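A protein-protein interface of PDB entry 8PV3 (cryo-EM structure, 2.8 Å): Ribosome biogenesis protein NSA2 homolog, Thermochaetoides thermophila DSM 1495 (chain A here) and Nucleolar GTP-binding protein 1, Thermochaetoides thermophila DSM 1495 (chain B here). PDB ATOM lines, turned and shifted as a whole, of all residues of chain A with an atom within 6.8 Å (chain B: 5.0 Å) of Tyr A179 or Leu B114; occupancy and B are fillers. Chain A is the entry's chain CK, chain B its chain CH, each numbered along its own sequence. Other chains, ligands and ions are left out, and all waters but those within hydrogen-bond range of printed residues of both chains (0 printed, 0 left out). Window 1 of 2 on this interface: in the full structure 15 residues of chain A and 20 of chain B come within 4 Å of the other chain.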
ATOM      1  N   LYS A 153      -9.000 -20.357   6.603  1.00  0.00           N
ATOM      2  CA  LYS A 153      -7.626 -19.995   6.304  1.00  0.00           C
ATOM      3  C   LYS A 153      -7.096 -20.873   5.176  1.00  0.00           C
ATOM      4  O   LYS A 153      -7.676 -21.923   4.877  1.00  0.00           O
ATOM      5  CB  LYS A 153      -6.748 -20.151   7.555  1.00  0.00           C
ATOM      6  CG  LYS A 153      -7.312 -19.490   8.793  1.00  0.00           C
ATOM      7  CD  LYS A 153      -7.041 -18.006   8.832  1.00  0.00           C
ATOM      8  CE  LYS A 153      -7.467 -17.423  10.165  1.00  0.00           C
ATOM      9  NZ  LYS A 153      -7.177 -15.968  10.258  1.00  0.00           N
ATOM     10  N   PRO A 154      -6.030 -20.447   4.490  1.00  0.00           N
ATOM     11  CA  PRO A 154      -5.431 -21.303   3.458  1.00  0.00           C
ATOM     12  C   PRO A 154      -4.902 -22.615   4.019  1.00  0.00           C
ATOM     13  O   PRO A 154      -4.378 -22.672   5.132  1.00  0.00           O
ATOM     14  CB  PRO A 154      -4.298 -20.437   2.903  1.00  0.00           C
ATOM     15  CG  PRO A 154      -4.756 -19.058   3.128  1.00  0.00           C
ATOM     16  CD  PRO A 154      -5.494 -19.075   4.425  1.00  0.00           C
ATOM     17  N   THR A 155      -5.049 -23.678   3.230  1.00  0.00           N
ATOM     18  CA  THR A 155      -4.637 -25.014   3.635  1.00  0.00           C
ATOM     19  C   THR A 155      -3.801 -25.654   2.538  1.00  0.00           C
ATOM     20  O   THR A 155      -3.866 -25.270   1.369  1.00  0.00           O
ATOM     21  CB  THR A 155      -5.832 -25.933   3.946  1.00  0.00           C
ATOM     22  OG1 THR A 155      -6.619 -26.113   2.764  1.00  0.00           O
ATOM     23  CG2 THR A 155      -6.697 -25.370   5.061  1.00  0.00           C
ATOM     24  N   PHE A 156      -3.000 -26.634   2.943  1.00  0.00           N
ATOM     25  CA  PHE A 156      -2.286 -27.520   2.033  1.00  0.00           C
ATOM     26  C   PHE A 156      -2.820 -28.927   2.249  1.00  0.00           C
ATOM     27  O   PHE A 156      -2.634 -29.505   3.326  1.00  0.00           O
ATOM     28  CB  PHE A 156      -0.776 -27.454   2.275  1.00  0.00           C
ATOM     29  CG  PHE A 156       0.009 -28.488   1.525  1.00  0.00           C
ATOM     30  CD1 PHE A 156       0.297 -28.319   0.183  1.00  0.00           C
ATOM     31  CD2 PHE A 156       0.478 -29.620   2.166  1.00  0.00           C
ATOM     32  CE1 PHE A 156       1.023 -29.268  -0.506  1.00  0.00           C
ATOM     33  CE2 PHE A 156       1.198 -30.567   1.483  1.00  0.00           C
ATOM     34  CZ  PHE A 156       1.473 -30.393   0.146  1.00  0.00           C
ATOM     35  N   VAL A 157      -3.493 -29.476   1.235  1.00  0.00           N
ATOM     36  CA  VAL A 157      -4.172 -30.760   1.385  1.00  0.00           C
ATOM     37  C   VAL A 157      -3.300 -31.947   1.004  1.00  0.00           C
ATOM     38  O   VAL A 157      -3.705 -33.096   1.240  1.00  0.00           O
ATOM     39  CB  VAL A 157      -5.480 -30.802   0.567  1.00  0.00           C
ATOM     40  CG1 VAL A 157      -6.458 -29.769   1.085  1.00  0.00           C
ATOM     41  CG2 VAL A 157      -5.192 -30.585  -0.902  1.00  0.00           C
ATOM     42  N   GLY A 158      -2.122 -31.715   0.435  1.00  0.00           N
ATOM     43  CA  GLY A 158      -1.234 -32.789   0.066  1.00  0.00           C
ATOM     44  C   GLY A 158      -1.523 -33.331  -1.317  1.00  0.00           C
ATOM     45  O   GLY A 158      -2.451 -32.889  -2.000  1.00  0.00           O
ATOM     46  N   MET A 175     -11.779 -25.548  -2.130  1.00  0.00           N
ATOM     47  CA  MET A 175     -10.792 -25.692  -3.196  1.00  0.00           C
ATOM     48  C   MET A 175     -10.086 -24.377  -3.495  1.00  0.00           C
ATOM     49  O   MET A 175      -8.892 -24.363  -3.813  1.00  0.00           O
ATOM     50  CB  MET A 175     -11.469 -26.228  -4.456  1.00  0.00           C
ATOM     51  CG  MET A 175     -11.993 -27.642  -4.325  1.00  0.00           C
ATOM     52  SD  MET A 175     -12.729 -28.265  -5.846  1.00  0.00           S
ATOM     53  CE  MET A 175     -14.272 -27.361  -5.868  1.00  0.00           C
ATOM     54  N   GLY A 176     -10.806 -23.262  -3.392  1.00  0.00           N
ATOM     55  CA  GLY A 176     -10.222 -21.970  -3.695  1.00  0.00           C
ATOM     56  C   GLY A 176      -9.279 -21.440  -2.639  1.00  0.00           C
ATOM     57  O   GLY A 176      -8.603 -20.438  -2.889  1.00  0.00           O
ATOM     58  N   LEU A 177      -9.221 -22.078  -1.472  1.00  0.00           N
ATOM     59  CA  LEU A 177      -8.279 -21.709  -0.426  1.00  0.00           C
ATOM     60  C   LEU A 177      -7.088 -22.655  -0.345  1.00  0.00           C
ATOM     61  O   LEU A 177      -6.275 -22.529   0.574  1.00  0.00           O
ATOM     62  CB  LEU A 177      -8.988 -21.649   0.927  1.00  0.00           C
ATOM     63  CG  LEU A 177      -9.693 -20.339   1.270  1.00  0.00           C
ATOM     64  CD1 LEU A 177     -10.546 -20.505   2.508  1.00  0.00           C
ATOM     65  CD2 LEU A 177      -8.680 -19.233   1.471  1.00  0.00           C
ATOM     66  N   ARG A 178      -6.956 -23.592  -1.275  1.00  0.00           N
ATOM     67  CA  ARG A 178      -5.857 -24.547  -1.245  1.00  0.00           C
ATOM     68  C   ARG A 178      -4.647 -23.982  -1.975  1.00  0.00           C
ATOM     69  O   ARG A 178      -4.789 -23.333  -3.015  1.00  0.00           O
ATOM     70  CB  ARG A 178      -6.273 -25.879  -1.865  1.00  0.00           C
ATOM     71  CG  ARG A 178      -7.395 -26.572  -1.128  1.00  0.00           C
ATOM     72  CD  ARG A 178      -7.813 -27.834  -1.846  1.00  0.00           C
ATOM     73  NE  ARG A 178      -9.117 -28.303  -1.399  1.00  0.00           N
ATOM     74  CZ  ARG A 178      -9.801 -29.275  -1.982  1.00  0.00           C
ATOM     75  NH1 ARG A 178      -9.327 -29.916  -3.037  1.00  0.00           N
ATOM     76  NH2 ARG A 178     -10.993 -29.611  -1.498  1.00  0.00           N
ATOM     77  N   TYR A 179      -3.463 -24.237  -1.428  1.00  0.00           N
ATOM     78  CA  TYR A 179      -2.211 -23.760  -1.993  1.00  0.00           C
ATOM     79  C   TYR A 179      -1.260 -24.924  -2.221  1.00  0.00           C
ATOM     80  O   TYR A 179      -1.371 -25.973  -1.582  1.00  0.00           O
ATOM     81  CB  TYR A 179      -1.546 -22.721  -1.087  1.00  0.00           C
ATOM     82  CG  TYR A 179      -2.170 -21.354  -1.187  1.00  0.00           C
ATOM     83  CD1 TYR A 179      -3.334 -21.050  -0.502  1.00  0.00           C
ATOM     84  CD2 TYR A 179      -1.602 -20.370  -1.982  1.00  0.00           C
ATOM     85  CE1 TYR A 179      -3.911 -19.802  -0.598  1.00  0.00           C
ATOM     86  CE2 TYR A 179      -2.172 -19.120  -2.083  1.00  0.00           C
ATOM     87  CZ  TYR A 179      -3.327 -18.843  -1.387  1.00  0.00           C
ATOM     88  OH  TYR A 179      -3.900 -17.599  -1.484  1.00  0.00           O
ATOM     89  N   LYS A 180      -0.321 -24.724  -3.144  1.00  0.00           N
ATOM     90  CA  LYS A 180       0.645 -25.745  -3.511  1.00  0.00           C
ATOM     91  C   LYS A 180       2.075 -25.224  -3.590  1.00  0.00           C
ATOM     92  O   LYS A 180       3.008 -25.993  -3.335  1.00  0.00           O
ATOM     93  CB  LYS A 180       0.245 -26.375  -4.858  1.00  0.00           C
ATOM     94  CG  LYS A 180       1.129 -27.498  -5.369  1.00  0.00           C
ATOM     95  CD  LYS A 180       0.549 -28.123  -6.623  1.00  0.00           C
ATOM     96  CE  LYS A 180       0.675 -27.184  -7.812  1.00  0.00           C
ATOM     97  NZ  LYS A 180       2.095 -26.999  -8.225  1.00  0.00           N
ATOM     98  N   LYS A 181       2.274 -23.937  -3.869  1.00  0.00           N
ATOM     99  CA  LYS A 181       3.601 -23.347  -3.975  1.00  0.00           C
ATOM    100  C   LYS A 181       3.720 -22.182  -3.002  1.00  0.00           C
ATOM    101  O   LYS A 181       2.723 -21.619  -2.546  1.00  0.00           O
ATOM    102  CB  LYS A 181       3.892 -22.870  -5.402  1.00  0.00           C
ATOM    103  CG  LYS A 181       4.044 -23.987  -6.414  1.00  0.00           C
ATOM    104  CD  LYS A 181       4.254 -23.429  -7.807  1.00  0.00           C
ATOM    105  CE  LYS A 181       4.476 -24.531  -8.826  1.00  0.00           C
ATOM    106  NZ  LYS A 181       4.587 -23.975 -10.204  1.00  0.00           N
ATOM    107  N   ALA A 182       4.963 -21.826  -2.683  1.00  0.00           N
ATOM    108  CA  ALA A 182       5.234 -20.715  -1.784  1.00  0.00           C
ATOM    109  C   ALA A 182       6.499 -19.999  -2.230  1.00  0.00           C
ATOM    110  O   ALA A 182       7.426 -20.621  -2.750  1.00  0.00           O
ATOM    111  CB  ALA A 182       5.388 -21.185  -0.336  1.00  0.00           C
ATOM    112  N   ILE A 197       5.343 -26.909  -1.980  1.00  0.00           N
ATOM    113  CA  ILE A 197       5.198 -27.276  -0.578  1.00  0.00           C
ATOM    114  C   ILE A 197       5.073 -28.789  -0.489  1.00  0.00           C
ATOM    115  O   ILE A 197       4.257 -29.395  -1.192  1.00  0.00           O
ATOM    116  CB  ILE A 197       3.978 -26.584   0.051  1.00  0.00           C
ATOM    117  CG1 ILE A 197       4.094 -25.066  -0.089  1.00  0.00           C
ATOM    118  CG2 ILE A 197       3.841 -26.964   1.509  1.00  0.00           C
ATOM    119  CD1 ILE A 197       2.882 -24.312   0.398  1.00  0.00           C
ATOM    120  N   LEU A 215      -2.123 -23.142   6.707  1.00  0.00           N
ATOM    121  CA  LEU A 215      -0.964 -22.295   6.442  1.00  0.00           C
ATOM    122  C   LEU A 215      -1.244 -20.920   7.036  1.00  0.00           C
ATOM    123  O   LEU A 215      -1.993 -20.126   6.461  1.00  0.00           O
ATOM    124  CB  LEU A 215      -0.680 -22.208   4.946  1.00  0.00           C
ATOM    125  CG  LEU A 215      -0.501 -23.517   4.181  1.00  0.00           C
ATOM    126  CD1 LEU A 215      -0.646 -23.276   2.695  1.00  0.00           C
ATOM    127  CD2 LEU A 215       0.843 -24.136   4.489  1.00  0.00           C
ATOM    128  N   PRO A 249      -1.181 -15.491   4.954  1.00  0.00           N
ATOM    129  CA  PRO A 249      -1.711 -15.893   3.641  1.00  0.00           C
ATOM    130  C   PRO A 249      -3.172 -15.545   3.428  1.00  0.00           C
ATOM    131  O   PRO A 249      -3.561 -15.243   2.294  1.00  0.00           O
ATOM    132  CB  PRO A 249      -1.482 -17.410   3.629  1.00  0.00           C
ATOM    133  CG  PRO A 249      -0.398 -17.642   4.622  1.00  0.00           C
ATOM    134  CD  PRO A 249      -0.637 -16.637   5.698  1.00  0.00           C
ATOM    135  N   GLU A 250      -3.989 -15.559   4.483  1.00  0.00           N
ATOM    136  CA  GLU A 250      -5.402 -15.221   4.335  1.00  0.00           C
ATOM    137  C   GLU A 250      -5.598 -13.745   4.016  1.00  0.00           C
ATOM    138  O   GLU A 250      -6.594 -13.376   3.387  1.00  0.00           O
ATOM    139  CB  GLU A 250      -6.174 -15.606   5.600  1.00  0.00           C
ATOM    140  CG  GLU A 250      -5.783 -14.839   6.857  1.00  0.00           C
ATOM    141  CD  GLU A 250      -4.604 -15.457   7.587  1.00  0.00           C
ATOM    142  OE1 GLU A 250      -4.088 -16.494   7.125  1.00  0.00           O
ATOM    143  OE2 GLU A 250      -4.193 -14.903   8.626  1.00  0.00           O
ATOM    144  N   ASP A 252      -2.995 -11.904   2.436  1.00  0.00           N
ATOM    145  CA  ASP A 252      -2.121 -11.526   1.336  1.00  0.00           C
ATOM    146  C   ASP A 252      -2.393 -12.278   0.043  1.00  0.00           C
ATOM    147  O   ASP A 252      -1.957 -11.822  -1.018  1.00  0.00           O
ATOM    148  CB  ASP A 252      -0.660 -11.737   1.737  1.00  0.00           C
ATOM    149  CG  ASP A 252      -0.210 -10.768   2.803  1.00  0.00           C
ATOM    150  OD1 ASP A 252      -0.755  -9.646   2.848  1.00  0.00           O
ATOM    151  OD2 ASP A 252       0.675 -11.126   3.605  1.00  0.00           O
ATOM    152  N   GLY A 253      -3.083 -13.414   0.095  1.00  0.00           N
ATOM    153  CA  GLY A 253      -3.294 -14.196  -1.102  1.00  0.00           C
ATOM    154  C   GLY A 253      -2.092 -14.977  -1.574  1.00  0.00           C
ATOM    155  O   GLY A 253      -2.142 -15.562  -2.660  1.00  0.00           O
ATOM    156  N   CYS A 254      -1.013 -15.007  -0.797  1.00  0.00           N
ATOM    157  CA  CYS A 254       0.187 -15.740  -1.163  1.00  0.00           C
ATOM    158  C   CYS A 254       0.866 -16.223   0.108  1.00  0.00           C
ATOM    159  O   CYS A 254       0.643 -15.687   1.195  1.00  0.00           O
ATOM    160  CB  CYS A 254       1.147 -14.879  -1.990  1.00  0.00           C
ATOM    161  SG  CYS A 254       1.756 -13.405  -1.142  1.00  0.00           S
ATOM    162  N   VAL A 255       1.701 -17.245  -0.041  1.00  0.00           N
ATOM    163  CA  VAL A 255       2.465 -17.810   1.064  1.00  0.00           C
ATOM    164  C   VAL A 255       3.917 -17.396   0.883  1.00  0.00           C
ATOM    165  O   VAL A 255       4.551 -17.755  -0.115  1.00  0.00           O
ATOM    166  CB  VAL A 255       2.326 -19.339   1.129  1.00  0.00           C
ATOM    167  CG1 VAL A 255       3.056 -19.889   2.341  1.00  0.00           C
ATOM    168  CG2 VAL A 255       0.863 -19.732   1.165  1.00  0.00           C
ATOM    169  N   ASP B 110      -8.320 -14.962  -9.058  1.00  0.00           N
ATOM    170  CA  ASP B 110      -7.827 -15.542  -7.811  1.00  0.00           C
ATOM    171  C   ASP B 110      -8.326 -14.761  -6.601  1.00  0.00           C
ATOM    172  O   ASP B 110      -8.788 -15.346  -5.611  1.00  0.00           O
ATOM    173  CB  ASP B 110      -6.300 -15.582  -7.826  1.00  0.00           C
ATOM    174  CG  ASP B 110      -5.754 -16.537  -8.863  1.00  0.00           C
ATOM    175  OD1 ASP B 110      -6.527 -17.377  -9.368  1.00  0.00           O
ATOM    176  OD2 ASP B 110      -4.549 -16.449  -9.176  1.00  0.00           O
ATOM    177  N   TYR B 111      -8.277 -13.432  -6.675  1.00  0.00           N
ATOM    178  CA  TYR B 111      -8.670 -12.651  -5.512  1.00  0.00           C
ATOM    179  C   TYR B 111     -10.182 -12.595  -5.324  1.00  0.00           C
ATOM    180  O   TYR B 111     -10.641 -12.496  -4.185  1.00  0.00           O
ATOM    181  CB  TYR B 111      -8.060 -11.256  -5.589  1.00  0.00           C
ATOM    182  CG  TYR B 111      -6.636 -11.256  -5.083  1.00  0.00           C
ATOM    183  CD1 TYR B 111      -6.364 -11.135  -3.732  1.00  0.00           C
ATOM    184  CD2 TYR B 111      -5.569 -11.413  -5.952  1.00  0.00           C
ATOM    185  CE1 TYR B 111      -5.072 -11.156  -3.262  1.00  0.00           C
ATOM    186  CE2 TYR B 111      -4.271 -11.428  -5.491  1.00  0.00           C
ATOM    187  CZ  TYR B 111      -4.030 -11.297  -4.145  1.00  0.00           C
ATOM    188  OH  TYR B 111      -2.738 -11.317  -3.678  1.00  0.00           O
ATOM    189  N   VAL B 112     -10.970 -12.692  -6.397  1.00  0.00           N
ATOM    190  CA  VAL B 112     -12.416 -12.845  -6.230  1.00  0.00           C
ATOM    191  C   VAL B 112     -12.740 -14.177  -5.557  1.00  0.00           C
ATOM    192  O   VAL B 112     -13.599 -14.248  -4.662  1.00  0.00           O
ATOM    193  CB  VAL B 112     -13.132 -12.689  -7.585  1.00  0.00           C
ATOM    194  CG1 VAL B 112     -14.585 -13.095  -7.481  1.00  0.00           C
ATOM    195  CG2 VAL B 112     -13.066 -11.246  -8.044  1.00  0.00           C
ATOM    196  N   ARG B 113     -12.037 -15.246  -5.951  1.00  0.00           N
ATOM    197  CA  ARG B 113     -12.247 -16.544  -5.312  1.00  0.00           C
ATOM    198  C   ARG B 113     -11.878 -16.508  -3.832  1.00  0.00           C
ATOM    199  O   ARG B 113     -12.535 -17.154  -3.009  1.00  0.00           O
ATOM    200  CB  ARG B 113     -11.444 -17.615  -6.044  1.00  0.00           C
ATOM    201  CG  ARG B 113     -11.950 -19.029  -5.834  1.00  0.00           C
ATOM    202  CD  ARG B 113     -11.216 -20.018  -6.721  1.00  0.00           C
ATOM    203  NE  ARG B 113     -11.257 -19.638  -8.127  1.00  0.00           N
ATOM    204  CZ  ARG B 113     -10.200 -19.264  -8.834  1.00  0.00           C
ATOM    205  NH1 ARG B 113      -8.996 -19.198  -8.294  1.00  0.00           N
ATOM    206  NH2 ARG B 113     -10.358 -18.944 -10.115  1.00  0.00           N
ATOM    207  N   LEU B 114     -10.832 -15.760  -3.473  1.00  0.00           N
ATOM    208  CA  LEU B 114     -10.478 -15.620  -2.058  1.00  0.00           C
ATOM    209  C   LEU B 114     -11.483 -14.748  -1.304  1.00  0.00           C
ATOM    210  O   LEU B 114     -11.786 -15.000  -0.126  1.00  0.00           O
ATOM    211  CB  LEU B 114      -9.070 -15.045  -1.925  1.00  0.00           C
ATOM    212  CG  LEU B 114      -7.952 -15.915  -2.491  1.00  0.00           C
ATOM    213  CD1 LEU B 114      -6.637 -15.167  -2.464  1.00  0.00           C
ATOM    214  CD2 LEU B 114      -7.850 -17.223  -1.732  1.00  0.00           C
ATOM    215  N   LEU B 115     -12.000 -13.708  -1.961  1.00  0.00           N
ATOM    216  CA  LEU B 115     -12.973 -12.826  -1.327  1.00  0.00           C
ATOM    217  C   LEU B 115     -14.306 -13.526  -1.110  1.00  0.00           C
ATOM    218  O   LEU B 115     -15.122 -13.062  -0.307  1.00  0.00           O
ATOM    219  CB  LEU B 115     -13.162 -11.569  -2.175  1.00  0.00           C
ATOM    220  CG  LEU B 115     -12.108 -10.480  -1.989  1.00  0.00           C
ATOM    221  CD1 LEU B 115     -12.175  -9.467  -3.113  1.00  0.00           C
ATOM    222  CD2 LEU B 115     -12.304  -9.802  -0.656  1.00  0.00           C
ATOM    223  N   LYS B 116     -14.559 -14.617  -1.839  1.00  0.00           N
ATOM    224  CA  LYS B 116     -15.708 -15.458  -1.512  1.00  0.00           C
ATOM    225  C   LYS B 116     -15.619 -16.052  -0.112  1.00  0.00           C
ATOM    226  O   LYS B 116     -16.657 -16.284   0.515  1.00  0.00           O
ATOM    227  CB  LYS B 116     -15.862 -16.602  -2.513  1.00  0.00           C
ATOM    228  CG  LYS B 116     -16.167 -16.178  -3.931  1.00  0.00           C
ATOM    229  CD  LYS B 116     -16.722 -17.337  -4.747  1.00  0.00           C
ATOM    230  CE  LYS B 116     -15.909 -18.606  -4.561  1.00  0.00           C
ATOM    231  NZ  LYS B 116     -16.561 -19.772  -5.211  1.00  0.00           N
ATOM    232  N   TYR B 117     -14.412 -16.304   0.388  1.00  0.00           N
ATOM    233  CA  TYR B 117     -14.219 -16.938   1.684  1.00  0.00           C
ATOM    234  C   TYR B 117     -13.680 -15.993   2.744  1.00  0.00           C
ATOM    235  O   TYR B 117     -13.480 -16.424   3.885  1.00  0.00           O
ATOM    236  CB  TYR B 117     -13.275 -18.135   1.548  1.00  0.00           C
ATOM    237  CG  TYR B 117     -13.724 -19.150   0.533  1.00  0.00           C
ATOM    238  CD1 TYR B 117     -14.826 -19.954   0.774  1.00  0.00           C
ATOM    239  CD2 TYR B 117     -13.046 -19.307  -0.666  1.00  0.00           C
ATOM    240  CE1 TYR B 117     -15.243 -20.881  -0.150  1.00  0.00           C
ATOM    241  CE2 TYR B 117     -13.455 -20.234  -1.597  1.00  0.00           C
ATOM    242  CZ  TYR B 117     -14.554 -21.019  -1.332  1.00  0.00           C
ATOM    243  OH  TYR B 117     -14.968 -21.948  -2.254  1.00  0.00           O
ATOM    244  N   ALA B 118     -13.407 -14.736   2.399  1.00  0.00           N
ATOM    245  CA  ALA B 118     -12.995 -13.763   3.404  1.00  0.00           C
ATOM    246  C   ALA B 118     -14.103 -13.540   4.433  1.00  0.00           C
ATOM    247  O   ALA B 118     -15.293 -13.568   4.113  1.00  0.00           O
ATOM    248  CB  ALA B 118     -12.614 -12.446   2.741  1.00  0.00           C
ATOM    249  N   LEU B 127      -7.257  -8.134   1.047  1.00  0.00           N
ATOM    250  CA  LEU B 127      -7.299  -8.834  -0.235  1.00  0.00           C
ATOM    251  C   LEU B 127      -7.476  -7.866  -1.402  1.00  0.00           C
ATOM    252  O   LEU B 127      -6.843  -8.032  -2.455  1.00  0.00           O
ATOM    253  CB  LEU B 127      -8.413  -9.877  -0.229  1.00  0.00           C
ATOM    254  CG  LEU B 127      -8.183 -11.127   0.621  1.00  0.00           C
ATOM    255  CD1 LEU B 127      -9.447 -11.963   0.690  1.00  0.00           C
ATOM    256  CD2 LEU B 127      -7.025 -11.941   0.079  1.00  0.00           C
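The side-chain hydroxyl of Tyr B111 sits at hydrogen-bond distance from the backbone carbonyl oxygen of Asp A252, 2.8 Å away.
NZ of Lys A153 is in salt-bridge range of OE2 of Glu A250, at 3.6 Å.
The backbone NH (N) of Thr A155 is in hydrogen-bond range of the backbone carbonyl oxygen (O) of Leu A177 (3.1 Å).
O of Thr A155 is in hydrogen-bond range of N of Tyr A179, at 3.0 Å.
The side-chain hydroxyl (OH) of Tyr A179 sits at hydrogen-bond distance from the backbone carbonyl oxygen (O) of Gly A253, 2.9 Å away.
NH1 of Arg B113 lies within salt-bridge range of OD1 of Asp B110.
CD of Arg B113 touches CA of Gly A176, 3.7 Å away.
Leu B114 touches Gly A176.
CD2 of Leu A177 touches CD2 of Leu B114, at 3.9 Å.
CD1 of Leu A177 touches CB of Tyr B117 (3.7 Å).
Tyr A179 touches Leu B114.
CD2 of Leu B127 touches O of Glu A250, 3.6 Å away.
Gly A253 touches Tyr B111.
Gly A253 touches Leu B114.
Of chain B, only Leu B114 comes within 4 Å of Tyr A179.
Lys A181 touches none of the printed residues of chain B.
Of the printed residues of chain B, Gly A253 touches Tyr B111 (3.9 Å) and Leu B114 (3.7 Å).
Val A255 touches none of the printed residues of chain B.
Of the printed residues of chain A, Arg B113 touches Gly A176 (3.7 Å).
Leu B114 touches four residues of chain A.
Of the printed residues of chain A, Leu B127 touches Glu A250 (3.6 Å).
The nearest printed residue of chain B that does not touch Tyr A179 is Leu B127 (6.6 Å).
The nearest residue of chain A that does not touch Leu B114 is Pro A249 (5.7 Å).
Printed residues of chain B that touch a printed residue of chain A: Tyr B111, Arg B113, Leu B114, Tyr B117 and Leu B127.
Hydrophobic or aromatic side chains of chain B that line the printed part of chain A: Tyr B111, Leu B114, Tyr B117 and Leu B127.
Of the 22 printed residues of chain A, 6 touch a printed residue of chain B.
Printed residues of chain A that touch a printed residue of chain B: Gly A176, Leu A177, Tyr A179, Glu A250, Asp A252 and Gly A253.
Hydrophobic or aromatic side chains of chain A within 4 Å of the printed part of chain B: Leu A177 and Tyr A179.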
